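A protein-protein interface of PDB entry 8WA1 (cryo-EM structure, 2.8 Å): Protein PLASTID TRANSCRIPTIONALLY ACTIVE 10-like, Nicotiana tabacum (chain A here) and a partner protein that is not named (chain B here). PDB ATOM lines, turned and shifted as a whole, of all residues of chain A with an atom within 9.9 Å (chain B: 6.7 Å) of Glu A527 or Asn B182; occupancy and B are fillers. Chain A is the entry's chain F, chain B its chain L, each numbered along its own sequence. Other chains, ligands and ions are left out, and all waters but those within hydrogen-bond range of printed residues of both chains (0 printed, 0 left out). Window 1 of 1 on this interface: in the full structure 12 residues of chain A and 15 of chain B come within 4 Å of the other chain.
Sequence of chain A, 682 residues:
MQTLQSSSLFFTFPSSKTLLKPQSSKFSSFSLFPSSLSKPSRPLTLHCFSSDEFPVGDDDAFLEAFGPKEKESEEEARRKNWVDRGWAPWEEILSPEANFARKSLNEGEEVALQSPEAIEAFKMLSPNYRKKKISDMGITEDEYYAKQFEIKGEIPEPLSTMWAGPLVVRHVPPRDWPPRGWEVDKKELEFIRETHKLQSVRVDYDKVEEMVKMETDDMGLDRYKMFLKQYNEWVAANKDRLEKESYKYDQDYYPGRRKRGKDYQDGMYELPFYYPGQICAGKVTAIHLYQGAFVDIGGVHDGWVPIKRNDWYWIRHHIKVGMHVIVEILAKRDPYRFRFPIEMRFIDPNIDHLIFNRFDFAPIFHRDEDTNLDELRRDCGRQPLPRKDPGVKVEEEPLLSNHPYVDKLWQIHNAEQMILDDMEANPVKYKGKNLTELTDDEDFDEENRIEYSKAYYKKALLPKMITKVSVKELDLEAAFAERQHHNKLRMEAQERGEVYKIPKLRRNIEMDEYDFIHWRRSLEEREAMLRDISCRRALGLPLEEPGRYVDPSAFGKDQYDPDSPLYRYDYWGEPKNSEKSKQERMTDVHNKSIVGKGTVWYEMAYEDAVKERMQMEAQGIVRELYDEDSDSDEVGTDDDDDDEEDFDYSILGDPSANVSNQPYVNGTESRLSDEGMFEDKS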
ATOM      1  N   VAL A 394     -21.337  12.220   2.835  1.00  0.00           N
ATOM      2  CA  VAL A 394     -21.143  13.286   1.855  1.00  0.00           C
ATOM      3  C   VAL A 394     -19.752  13.895   1.968  1.00  0.00           C
ATOM      4  O   VAL A 394     -19.226  14.440   0.988  1.00  0.00           O
ATOM      5  CB  VAL A 394     -22.238  14.356   2.014  1.00  0.00           C
ATOM      6  N   GLU A 395     -19.136  13.829   3.150  1.00  0.00           N
ATOM      7  CA  GLU A 395     -17.806  14.408   3.319  1.00  0.00           C
ATOM      8  C   GLU A 395     -16.758  13.621   2.540  1.00  0.00           C
ATOM      9  O   GLU A 395     -15.895  14.209   1.877  1.00  0.00           O
ATOM     10  CB  GLU A 395     -17.442  14.464   4.803  1.00  0.00           C
ATOM     11  N   LEU A 399     -15.125  14.010  -5.942  1.00  0.00           N
ATOM     12  CA  LEU A 399     -15.587  15.308  -6.408  1.00  0.00           C
ATOM     13  C   LEU A 399     -16.176  15.197  -7.813  1.00  0.00           C
ATOM     14  O   LEU A 399     -15.922  14.244  -8.554  1.00  0.00           O
ATOM     15  CB  LEU A 399     -14.444  16.323  -6.401  1.00  0.00           C
ATOM     16  CG  LEU A 399     -14.179  17.101  -5.110  1.00  0.00           C
ATOM     17  CD1 LEU A 399     -13.720  16.184  -3.987  1.00  0.00           C
ATOM     18  CD2 LEU A 399     -13.156  18.199  -5.359  1.00  0.00           C
ATOM     19  N   TRP A 519     -14.770  21.912 -11.491  1.00  0.00           N
ATOM     20  CA  TRP A 519     -14.021  21.202 -10.460  1.00  0.00           C
ATOM     21  C   TRP A 519     -13.559  22.152  -9.362  1.00  0.00           C
ATOM     22  O   TRP A 519     -13.558  21.790  -8.182  1.00  0.00           O
ATOM     23  CB  TRP A 519     -12.828  20.476 -11.082  1.00  0.00           C
ATOM     24  CG  TRP A 519     -11.920  19.849 -10.072  1.00  0.00           C
ATOM     25  CD1 TRP A 519     -12.003  18.584  -9.566  1.00  0.00           C
ATOM     26  CD2 TRP A 519     -10.790  20.459  -9.438  1.00  0.00           C
ATOM     27  NE1 TRP A 519     -10.994  18.369  -8.660  1.00  0.00           N
ATOM     28  CE2 TRP A 519     -10.236  19.506  -8.563  1.00  0.00           C
ATOM     29  CE3 TRP A 519     -10.194  21.721  -9.528  1.00  0.00           C
ATOM     30  CZ2 TRP A 519      -9.115  19.774  -7.781  1.00  0.00           C
ATOM     31  CZ3 TRP A 519      -9.081  21.984  -8.752  1.00  0.00           C
ATOM     32  CH2 TRP A 519      -8.554  21.015  -7.890  1.00  0.00           C
ATOM     33  N   ARG A 520     -13.153  23.369  -9.734  1.00  0.00           N
ATOM     34  CA  ARG A 520     -12.787  24.365  -8.729  1.00  0.00           C
ATOM     35  C   ARG A 520     -13.977  24.710  -7.843  1.00  0.00           C
ATOM     36  O   ARG A 520     -13.837  24.829  -6.619  1.00  0.00           O
ATOM     37  CB  ARG A 520     -12.248  25.629  -9.398  1.00  0.00           C
ATOM     38  CG  ARG A 520     -10.871  25.495 -10.022  1.00  0.00           C
ATOM     39  CD  ARG A 520     -10.201  26.858 -10.109  1.00  0.00           C
ATOM     40  NE  ARG A 520     -11.113  27.879 -10.618  1.00  0.00           N
ATOM     41  CZ  ARG A 520     -10.869  29.186 -10.585  1.00  0.00           C
ATOM     42  NH1 ARG A 520     -11.758  30.041 -11.071  1.00  0.00           N
ATOM     43  NH2 ARG A 520      -9.738  29.639 -10.060  1.00  0.00           N
ATOM     44  N   ARG A 521     -15.154  24.888  -8.448  1.00  0.00           N
ATOM     45  CA  ARG A 521     -16.354  25.174  -7.667  1.00  0.00           C
ATOM     46  C   ARG A 521     -16.659  24.040  -6.697  1.00  0.00           C
ATOM     47  O   ARG A 521     -16.948  24.275  -5.517  1.00  0.00           O
ATOM     48  CB  ARG A 521     -17.539  25.421  -8.602  1.00  0.00           C
ATOM     49  CG  ARG A 521     -18.830  25.784  -7.886  1.00  0.00           C
ATOM     50  CD  ARG A 521     -19.935  26.117  -8.878  1.00  0.00           C
ATOM     51  NE  ARG A 521     -21.147  26.590  -8.213  1.00  0.00           N
ATOM     52  CZ  ARG A 521     -22.207  25.830  -7.956  1.00  0.00           C
ATOM     53  NH1 ARG A 521     -23.263  26.351  -7.347  1.00  0.00           N
ATOM     54  NH2 ARG A 521     -22.213  24.553  -8.311  1.00  0.00           N
ATOM     55  N   SER A 522     -16.595  22.796  -7.181  1.00  0.00           N
ATOM     56  CA  SER A 522     -16.863  21.651  -6.314  1.00  0.00           C
ATOM     57  C   SER A 522     -15.836  21.548  -5.192  1.00  0.00           C
ATOM     58  O   SER A 522     -16.186  21.234  -4.046  1.00  0.00           O
ATOM     59  CB  SER A 522     -16.886  20.365  -7.139  1.00  0.00           C
ATOM     60  OG  SER A 522     -17.046  19.230  -6.306  1.00  0.00           O
ATOM     61  N   LEU A 523     -14.563  21.808  -5.502  1.00  0.00           N
ATOM     62  CA  LEU A 523     -13.520  21.748  -4.485  1.00  0.00           C
ATOM     63  C   LEU A 523     -13.731  22.813  -3.420  1.00  0.00           C
ATOM     64  O   LEU A 523     -13.563  22.546  -2.224  1.00  0.00           O
ATOM     65  CB  LEU A 523     -12.145  21.906  -5.133  1.00  0.00           C
ATOM     66  CG  LEU A 523     -10.954  21.946  -4.170  1.00  0.00           C
ATOM     67  CD1 LEU A 523     -10.741  20.588  -3.517  1.00  0.00           C
ATOM     68  CD2 LEU A 523      -9.694  22.412  -4.882  1.00  0.00           C
ATOM     69  N   GLU A 524     -14.098  24.029  -3.830  1.00  0.00           N
ATOM     70  CA  GLU A 524     -14.361  25.083  -2.857  1.00  0.00           C
ATOM     71  C   GLU A 524     -15.573  24.742  -2.000  1.00  0.00           C
ATOM     72  O   GLU A 524     -15.578  24.982  -0.786  1.00  0.00           O
ATOM     73  CB  GLU A 524     -14.559  26.420  -3.574  1.00  0.00           C
ATOM     74  CG  GLU A 524     -14.695  27.608  -2.639  1.00  0.00           C
ATOM     75  CD  GLU A 524     -14.729  28.931  -3.376  1.00  0.00           C
ATOM     76  OE1 GLU A 524     -14.436  28.946  -4.590  1.00  0.00           O
ATOM     77  OE2 GLU A 524     -15.050  29.958  -2.741  1.00  0.00           O
ATOM     78  N   GLU A 525     -16.610  24.167  -2.616  1.00  0.00           N
ATOM     79  CA  GLU A 525     -17.783  23.738  -1.862  1.00  0.00           C
ATOM     80  C   GLU A 525     -17.407  22.707  -0.802  1.00  0.00           C
ATOM     81  O   GLU A 525     -17.812  22.815   0.358  1.00  0.00           O
ATOM     82  CB  GLU A 525     -18.849  23.180  -2.807  1.00  0.00           C
ATOM     83  CG  GLU A 525     -19.956  22.415  -2.093  1.00  0.00           C
ATOM     84  CD  GLU A 525     -21.157  22.148  -2.980  1.00  0.00           C
ATOM     85  OE1 GLU A 525     -21.573  23.069  -3.710  1.00  0.00           O
ATOM     86  OE2 GLU A 525     -21.685  21.016  -2.946  1.00  0.00           O
ATOM     87  N   ARG A 526     -16.623  21.697  -1.187  1.00  0.00           N
ATOM     88  CA  ARG A 526     -16.227  20.668  -0.227  1.00  0.00           C
ATOM     89  C   ARG A 526     -15.303  21.223   0.854  1.00  0.00           C
ATOM     90  O   ARG A 526     -15.392  20.813   2.021  1.00  0.00           O
ATOM     91  CB  ARG A 526     -15.559  19.500  -0.953  1.00  0.00           C
ATOM     92  CG  ARG A 526     -15.082  18.389  -0.032  1.00  0.00           C
ATOM     93  CD  ARG A 526     -15.240  17.019  -0.672  1.00  0.00           C
ATOM     94  NE  ARG A 526     -16.643  16.626  -0.784  1.00  0.00           N
ATOM     95  CZ  ARG A 526     -17.364  16.727  -1.897  1.00  0.00           C
ATOM     96  NH1 ARG A 526     -16.816  17.206  -3.004  1.00  0.00           N
ATOM     97  NH2 ARG A 526     -18.634  16.346  -1.902  1.00  0.00           N
ATOM     98  N   GLU A 527     -14.415  22.151   0.494  1.00  0.00           N
ATOM     99  CA  GLU A 527     -13.523  22.745   1.485  1.00  0.00           C
ATOM    100  C   GLU A 527     -14.306  23.558   2.506  1.00  0.00           C
ATOM    101  O   GLU A 527     -13.999  23.527   3.703  1.00  0.00           O
ATOM    102  CB  GLU A 527     -12.473  23.612   0.794  1.00  0.00           C
ATOM    103  CG  GLU A 527     -11.380  24.116   1.719  1.00  0.00           C
ATOM    104  CD  GLU A 527     -10.261  24.815   0.972  1.00  0.00           C
ATOM    105  OE1 GLU A 527     -10.433  25.101  -0.231  1.00  0.00           O
ATOM    106  OE2 GLU A 527      -9.206  25.072   1.588  1.00  0.00           O
ATOM    107  N   ALA A 528     -15.324  24.293   2.051  1.00  0.00           N
ATOM    108  CA  ALA A 528     -16.196  24.992   2.989  1.00  0.00           C
ATOM    109  C   ALA A 528     -17.035  24.010   3.797  1.00  0.00           C
ATOM    110  O   ALA A 528     -17.342  24.263   4.968  1.00  0.00           O
ATOM    111  CB  ALA A 528     -17.092  25.977   2.239  1.00  0.00           C
ATOM    112  N   MET A 529     -17.409  22.882   3.189  1.00  0.00           N
ATOM    113  CA  MET A 529     -18.233  21.896   3.878  1.00  0.00           C
ATOM    114  C   MET A 529     -17.477  21.252   5.031  1.00  0.00           C
ATOM    115  O   MET A 529     -18.063  20.953   6.076  1.00  0.00           O
ATOM    116  CB  MET A 529     -18.713  20.834   2.889  1.00  0.00           C
ATOM    117  CG  MET A 529     -19.645  19.796   3.487  1.00  0.00           C
ATOM    118  SD  MET A 529     -20.114  18.520   2.304  1.00  0.00           S
ATOM    119  CE  MET A 529     -18.514  17.815   1.920  1.00  0.00           C
ATOM    120  N   LEU A 530     -16.175  21.018   4.855  1.00  0.00           N
ATOM    121  CA  LEU A 530     -15.380  20.464   5.949  1.00  0.00           C
ATOM    122  C   LEU A 530     -15.388  21.392   7.162  1.00  0.00           C
ATOM    123  O   LEU A 530     -15.644  20.954   8.294  1.00  0.00           O
ATOM    124  CB  LEU A 530     -13.950  20.200   5.481  1.00  0.00           C
ATOM    125  CG  LEU A 530     -13.793  19.169   4.360  1.00  0.00           C
ATOM    126  CD1 LEU A 530     -12.334  19.020   3.961  1.00  0.00           C
ATOM    127  CD2 LEU A 530     -14.379  17.829   4.777  1.00  0.00           C
ATOM    128  N   ARG A 531     -15.127  22.684   6.940  1.00  0.00           N
ATOM    129  CA  ARG A 531     -15.148  23.641   8.041  1.00  0.00           C
ATOM    130  C   ARG A 531     -16.542  23.753   8.644  1.00  0.00           C
ATOM    131  O   ARG A 531     -16.687  23.907   9.862  1.00  0.00           O
ATOM    132  CB  ARG A 531     -14.669  25.012   7.566  1.00  0.00           C
ATOM    133  CG  ARG A 531     -13.265  25.040   6.991  1.00  0.00           C
ATOM    134  CD  ARG A 531     -12.854  26.469   6.669  1.00  0.00           C
ATOM    135  NE  ARG A 531     -13.833  27.130   5.810  1.00  0.00           N
ATOM    136  CZ  ARG A 531     -13.835  28.431   5.541  1.00  0.00           C
ATOM    137  NH1 ARG A 531     -12.911  29.222   6.066  1.00  0.00           N
ATOM    138  NH2 ARG A 531     -14.767  28.942   4.747  1.00  0.00           N
ATOM    139  N   ASP A 532     -17.580  23.679   7.808  1.00  0.00           N
ATOM    140  CA  ASP A 532     -18.942  23.777   8.319  1.00  0.00           C
ATOM    141  C   ASP A 532     -19.283  22.589   9.208  1.00  0.00           C
ATOM    142  O   ASP A 532     -19.904  22.754  10.265  1.00  0.00           O
ATOM    143  CB  ASP A 532     -19.931  23.883   7.160  1.00  0.00           C
ATOM    144  CG  ASP A 532     -21.339  24.206   7.622  1.00  0.00           C
ATOM    145  OD1 ASP A 532     -21.522  24.514   8.819  1.00  0.00           O
ATOM    146  OD2 ASP A 532     -22.266  24.151   6.788  1.00  0.00           O
ATOM    147  N   ILE A 533     -18.735  21.435   8.844  1.00  0.00           N
ATOM    148  CA  ILE A 533     -18.955  20.234   9.633  1.00  0.00           C
ATOM    149  C   ILE A 533     -18.361  20.494  10.982  1.00  0.00           C
ATOM    150  O   ILE A 533     -19.010  20.298  11.997  1.00  0.00           O
ATOM    151  CB  ILE A 533     -18.268  19.001   9.004  1.00  0.00           C
ATOM    152  CG1 ILE A 533     -19.083  18.444   7.836  1.00  0.00           C
ATOM    153  CG2 ILE A 533     -18.057  17.888  10.020  1.00  0.00           C
ATOM    154  CD1 ILE A 533     -20.558  18.776   7.869  1.00  0.00           C
ATOM    155  N   SER A 534     -17.140  20.995  11.006  1.00  0.00           N
ATOM    156  CA  SER A 534     -16.480  21.162  12.284  1.00  0.00           C
ATOM    157  C   SER A 534     -17.206  22.151  13.127  1.00  0.00           C
ATOM    158  O   SER A 534     -17.503  21.881  14.273  1.00  0.00           O
ATOM    159  CB  SER A 534     -15.057  21.631  12.102  1.00  0.00           C
ATOM    160  OG  SER A 534     -14.533  22.110  13.325  1.00  0.00           O
ATOM    161  N   CYS A 535     -17.483  23.307  12.558  1.00  0.00           N
ATOM    162  CA  CYS A 535     -18.179  24.323  13.300  1.00  0.00           C
ATOM    163  C   CYS A 535     -19.458  23.782  13.888  1.00  0.00           C
ATOM    164  O   CYS A 535     -19.744  24.019  15.057  1.00  0.00           O
ATOM    165  CB  CYS A 535     -18.526  25.490  12.389  1.00  0.00           C
ATOM    166  SG  CYS A 535     -17.130  26.502  11.866  1.00  0.00           S
ATOM    167  N   TYR B 179      -2.184  30.252   6.160  1.00  0.00           N
ATOM    168  CA  TYR B 179      -1.659  30.065   4.816  1.00  0.00           C
ATOM    169  C   TYR B 179      -2.196  28.748   4.278  1.00  0.00           C
ATOM    170  O   TYR B 179      -1.845  27.676   4.784  1.00  0.00           O
ATOM    171  CB  TYR B 179      -0.129  30.074   4.824  1.00  0.00           C
ATOM    172  CG  TYR B 179       0.522  29.628   3.534  1.00  0.00           C
ATOM    173  CD1 TYR B 179       0.629  30.490   2.450  1.00  0.00           C
ATOM    174  CD2 TYR B 179       1.052  28.351   3.409  1.00  0.00           C
ATOM    175  CE1 TYR B 179       1.232  30.087   1.272  1.00  0.00           C
ATOM    176  CE2 TYR B 179       1.656  27.939   2.238  1.00  0.00           C
ATOM    177  CZ  TYR B 179       1.745  28.809   1.173  1.00  0.00           C
ATOM    178  OH  TYR B 179       2.348  28.396   0.008  1.00  0.00           O
ATOM    179  N   LYS B 180      -3.044  28.831   3.259  1.00  0.00           N
ATOM    180  CA  LYS B 180      -3.851  27.701   2.818  1.00  0.00           C
ATOM    181  C   LYS B 180      -3.011  26.780   1.943  1.00  0.00           C
ATOM    182  O   LYS B 180      -2.776  27.076   0.767  1.00  0.00           O
ATOM    183  CB  LYS B 180      -5.085  28.183   2.056  1.00  0.00           C
ATOM    184  CG  LYS B 180      -5.978  27.064   1.551  1.00  0.00           C
ATOM    185  CD  LYS B 180      -7.219  27.617   0.870  1.00  0.00           C
ATOM    186  CE  LYS B 180      -6.856  28.481  -0.325  1.00  0.00           C
ATOM    187  NZ  LYS B 180      -8.069  29.012  -1.008  1.00  0.00           N
ATOM    188  N   ALA B 181      -2.567  25.657   2.523  1.00  0.00           N
ATOM    189  CA  ALA B 181      -1.892  24.593   1.791  1.00  0.00           C
ATOM    190  C   ALA B 181      -2.531  23.273   2.231  1.00  0.00           C
ATOM    191  O   ALA B 181      -2.071  22.590   3.143  1.00  0.00           O
ATOM    192  CB  ALA B 181      -0.382  24.602   2.036  1.00  0.00           C
ATOM    193  N   ASN B 182      -3.621  22.907   1.562  1.00  0.00           N
ATOM    194  CA  ASN B 182      -4.397  21.729   1.917  1.00  0.00           C
ATOM    195  C   ASN B 182      -4.361  20.707   0.790  1.00  0.00           C
ATOM    196  O   ASN B 182      -4.300  21.066  -0.390  1.00  0.00           O
ATOM    197  CB  ASN B 182      -5.846  22.108   2.234  1.00  0.00           C
ATOM    198  CG  ASN B 182      -6.543  22.774   1.067  1.00  0.00           C
ATOM    199  OD1 ASN B 182      -5.923  23.494   0.285  1.00  0.00           O
ATOM    200  ND2 ASN B 182      -7.843  22.535   0.941  1.00  0.00           N
ATOM    201  N   ARG B 183      -4.390  19.431   1.163  1.00  0.00           N
ATOM    202  CA  ARG B 183      -4.426  18.323   0.214  1.00  0.00           C
ATOM    203  C   ARG B 183      -5.550  17.384   0.632  1.00  0.00           C
ATOM    204  O   ARG B 183      -5.474  16.756   1.693  1.00  0.00           O
ATOM    205  CB  ARG B 183      -3.084  17.595   0.166  1.00  0.00           C
ATOM    206  N   LEU B 184      -6.591  17.302  -0.188  1.00  0.00           N
ATOM    207  CA  LEU B 184      -7.747  16.482   0.131  1.00  0.00           C
ATOM    208  C   LEU B 184      -7.478  15.013  -0.184  1.00  0.00           C
ATOM    209  O   LEU B 184      -6.623  14.669  -1.005  1.00  0.00           O
ATOM    210  CB  LEU B 184      -8.976  16.964  -0.636  1.00  0.00           C
ATOM    211  N   THR B 189      -8.629  15.300  -5.912  1.00  0.00           N
ATOM    212  CA  THR B 189      -8.035  16.363  -5.109  1.00  0.00           C
ATOM    213  C   THR B 189      -6.981  17.131  -5.898  1.00  0.00           C
ATOM    214  O   THR B 189      -6.817  18.342  -5.707  1.00  0.00           O
ATOM    215  CB  THR B 189      -7.414  15.785  -3.823  1.00  0.00           C
ATOM    216  N   ASP B 198      -2.651  29.528  -5.862  1.00  0.00           N
ATOM    217  CA  ASP B 198      -3.447  28.446  -5.290  1.00  0.00           C
ATOM    218  C   ASP B 198      -3.351  28.448  -3.771  1.00  0.00           C
ATOM    219  O   ASP B 198      -4.368  28.340  -3.077  1.00  0.00           O
ATOM    220  CB  ASP B 198      -2.994  27.101  -5.860  1.00  0.00           C
ATOM    221  N   TRP B 215      -8.125  21.249   9.561  1.00  0.00           N
ATOM    222  CA  TRP B 215      -8.393  21.128   8.146  1.00  0.00           C
ATOM    223  C   TRP B 215      -7.132  21.323   7.324  1.00  0.00           C
ATOM    224  O   TRP B 215      -7.188  22.002   6.302  1.00  0.00           O
ATOM    225  CB  TRP B 215      -9.550  22.025   7.692  1.00  0.00           C
ATOM    226  CG  TRP B 215      -9.683  23.318   8.401  1.00  0.00           C
ATOM    227  CD1 TRP B 215      -8.876  24.383   8.274  1.00  0.00           C
ATOM    228  CD2 TRP B 215     -10.709  23.700   9.322  1.00  0.00           C
ATOM    229  NE1 TRP B 215      -9.312  25.417   9.055  1.00  0.00           N
ATOM    230  CE2 TRP B 215     -10.439  25.021   9.718  1.00  0.00           C
ATOM    231  CE3 TRP B 215     -11.825  23.057   9.852  1.00  0.00           C
ATOM    232  CZ2 TRP B 215     -11.237  25.709  10.619  1.00  0.00           C
ATOM    233  CZ3 TRP B 215     -12.613  23.743  10.749  1.00  0.00           C
ATOM    234  CH2 TRP B 215     -12.320  25.055  11.121  1.00  0.00           C
ATOM    235  N   ASP B 216      -6.014  20.732   7.763  1.00  0.00           N
ATOM    236  CA  ASP B 216      -4.751  20.800   7.023  1.00  0.00           C
ATOM    237  C   ASP B 216      -4.277  22.225   6.766  1.00  0.00           C
ATOM    238  O   ASP B 216      -3.351  22.419   5.963  1.00  0.00           O
ATOM    239  CB  ASP B 216      -4.830  20.053   5.686  1.00  0.00           C
ATOM    240  CG  ASP B 216      -3.484  19.507   5.242  1.00  0.00           C
ATOM    241  OD1 ASP B 216      -2.513  19.613   6.021  1.00  0.00           O
ATOM    242  OD2 ASP B 216      -3.399  18.974   4.116  1.00  0.00           O
ATOM    243  N   TYR B 217      -4.870  23.230   7.404  1.00  0.00           N
ATOM    244  CA  TYR B 217      -4.376  24.589   7.247  1.00  0.00           C
ATOM    245  C   TYR B 217      -3.159  24.819   8.140  1.00  0.00           C
ATOM    246  O   TYR B 217      -2.889  24.064   9.079  1.00  0.00           O
ATOM    247  CB  TYR B 217      -5.467  25.612   7.575  1.00  0.00           C
ATOM    248  CG  TYR B 217      -6.504  25.802   6.486  1.00  0.00           C
ATOM    249  CD1 TYR B 217      -6.526  24.985   5.362  1.00  0.00           C
ATOM    250  CD2 TYR B 217      -7.453  26.811   6.579  1.00  0.00           C
ATOM    251  CE1 TYR B 217      -7.474  25.163   4.369  1.00  0.00           C
ATOM    252  CE2 TYR B 217      -8.402  26.997   5.590  1.00  0.00           C
ATOM    253  CZ  TYR B 217      -8.407  26.170   4.488  1.00  0.00           C
ATOM    254  OH  TYR B 217      -9.350  26.353   3.503  1.00  0.00           O
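The side-chain amide nitrogen (ND2) of Asn B182 is in hydrogen-bond range of the side-chain carboxylate (OE2) of Glu A527, 3.0 Å away. The side-chain hydroxyl (OH) of Tyr B217 lies close to the side-chain carboxylate (OE2) of Glu A527.
SG of Cys A535 lies within hydrogen-bond range of O of Arg A531 (3.3 Å).
Among the printed residues, merely in contact across the chains: Glu A527 with Lys B180, Trp A519 with Thr B189, Ser A534 with Trp B215 and Arg A531 with Trp B215.
Glu A527 touches just these residues of chain B: Lys B180, Asn B182 and Tyr B217. Asn B182 touches just one residue of chain A: Glu A527 (3.0 Å). No residue of chain A comes within 4 Å of Asp B216. Of the printed residues of chain B, Arg A531 touches Trp B215. Printed residues of chain A within 4 Å of Thr B189: Trp A519 (3.4 Å). Printed residues of chain A within 4 Å of Lys B180: Glu A527 (3.3 Å). The nearest printed residue of chain A that does not touch Lys B180 is Glu A524 (7.0 Å).
Of the 20 printed residues of chain A, 4 touch a printed residue of chain B. Hydrophobic or aromatic side chains of chain A that line the printed part of chain B: Trp A519. Along chain A the printed residues that touch a printed residue of chain B span positions 519 to 534. Hydrophobic or aromatic side chains of chain B within 4 Å of the printed part of chain A: Trp B215 and Tyr B217. Among the printed residues, 6 pairs touch across the chains.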
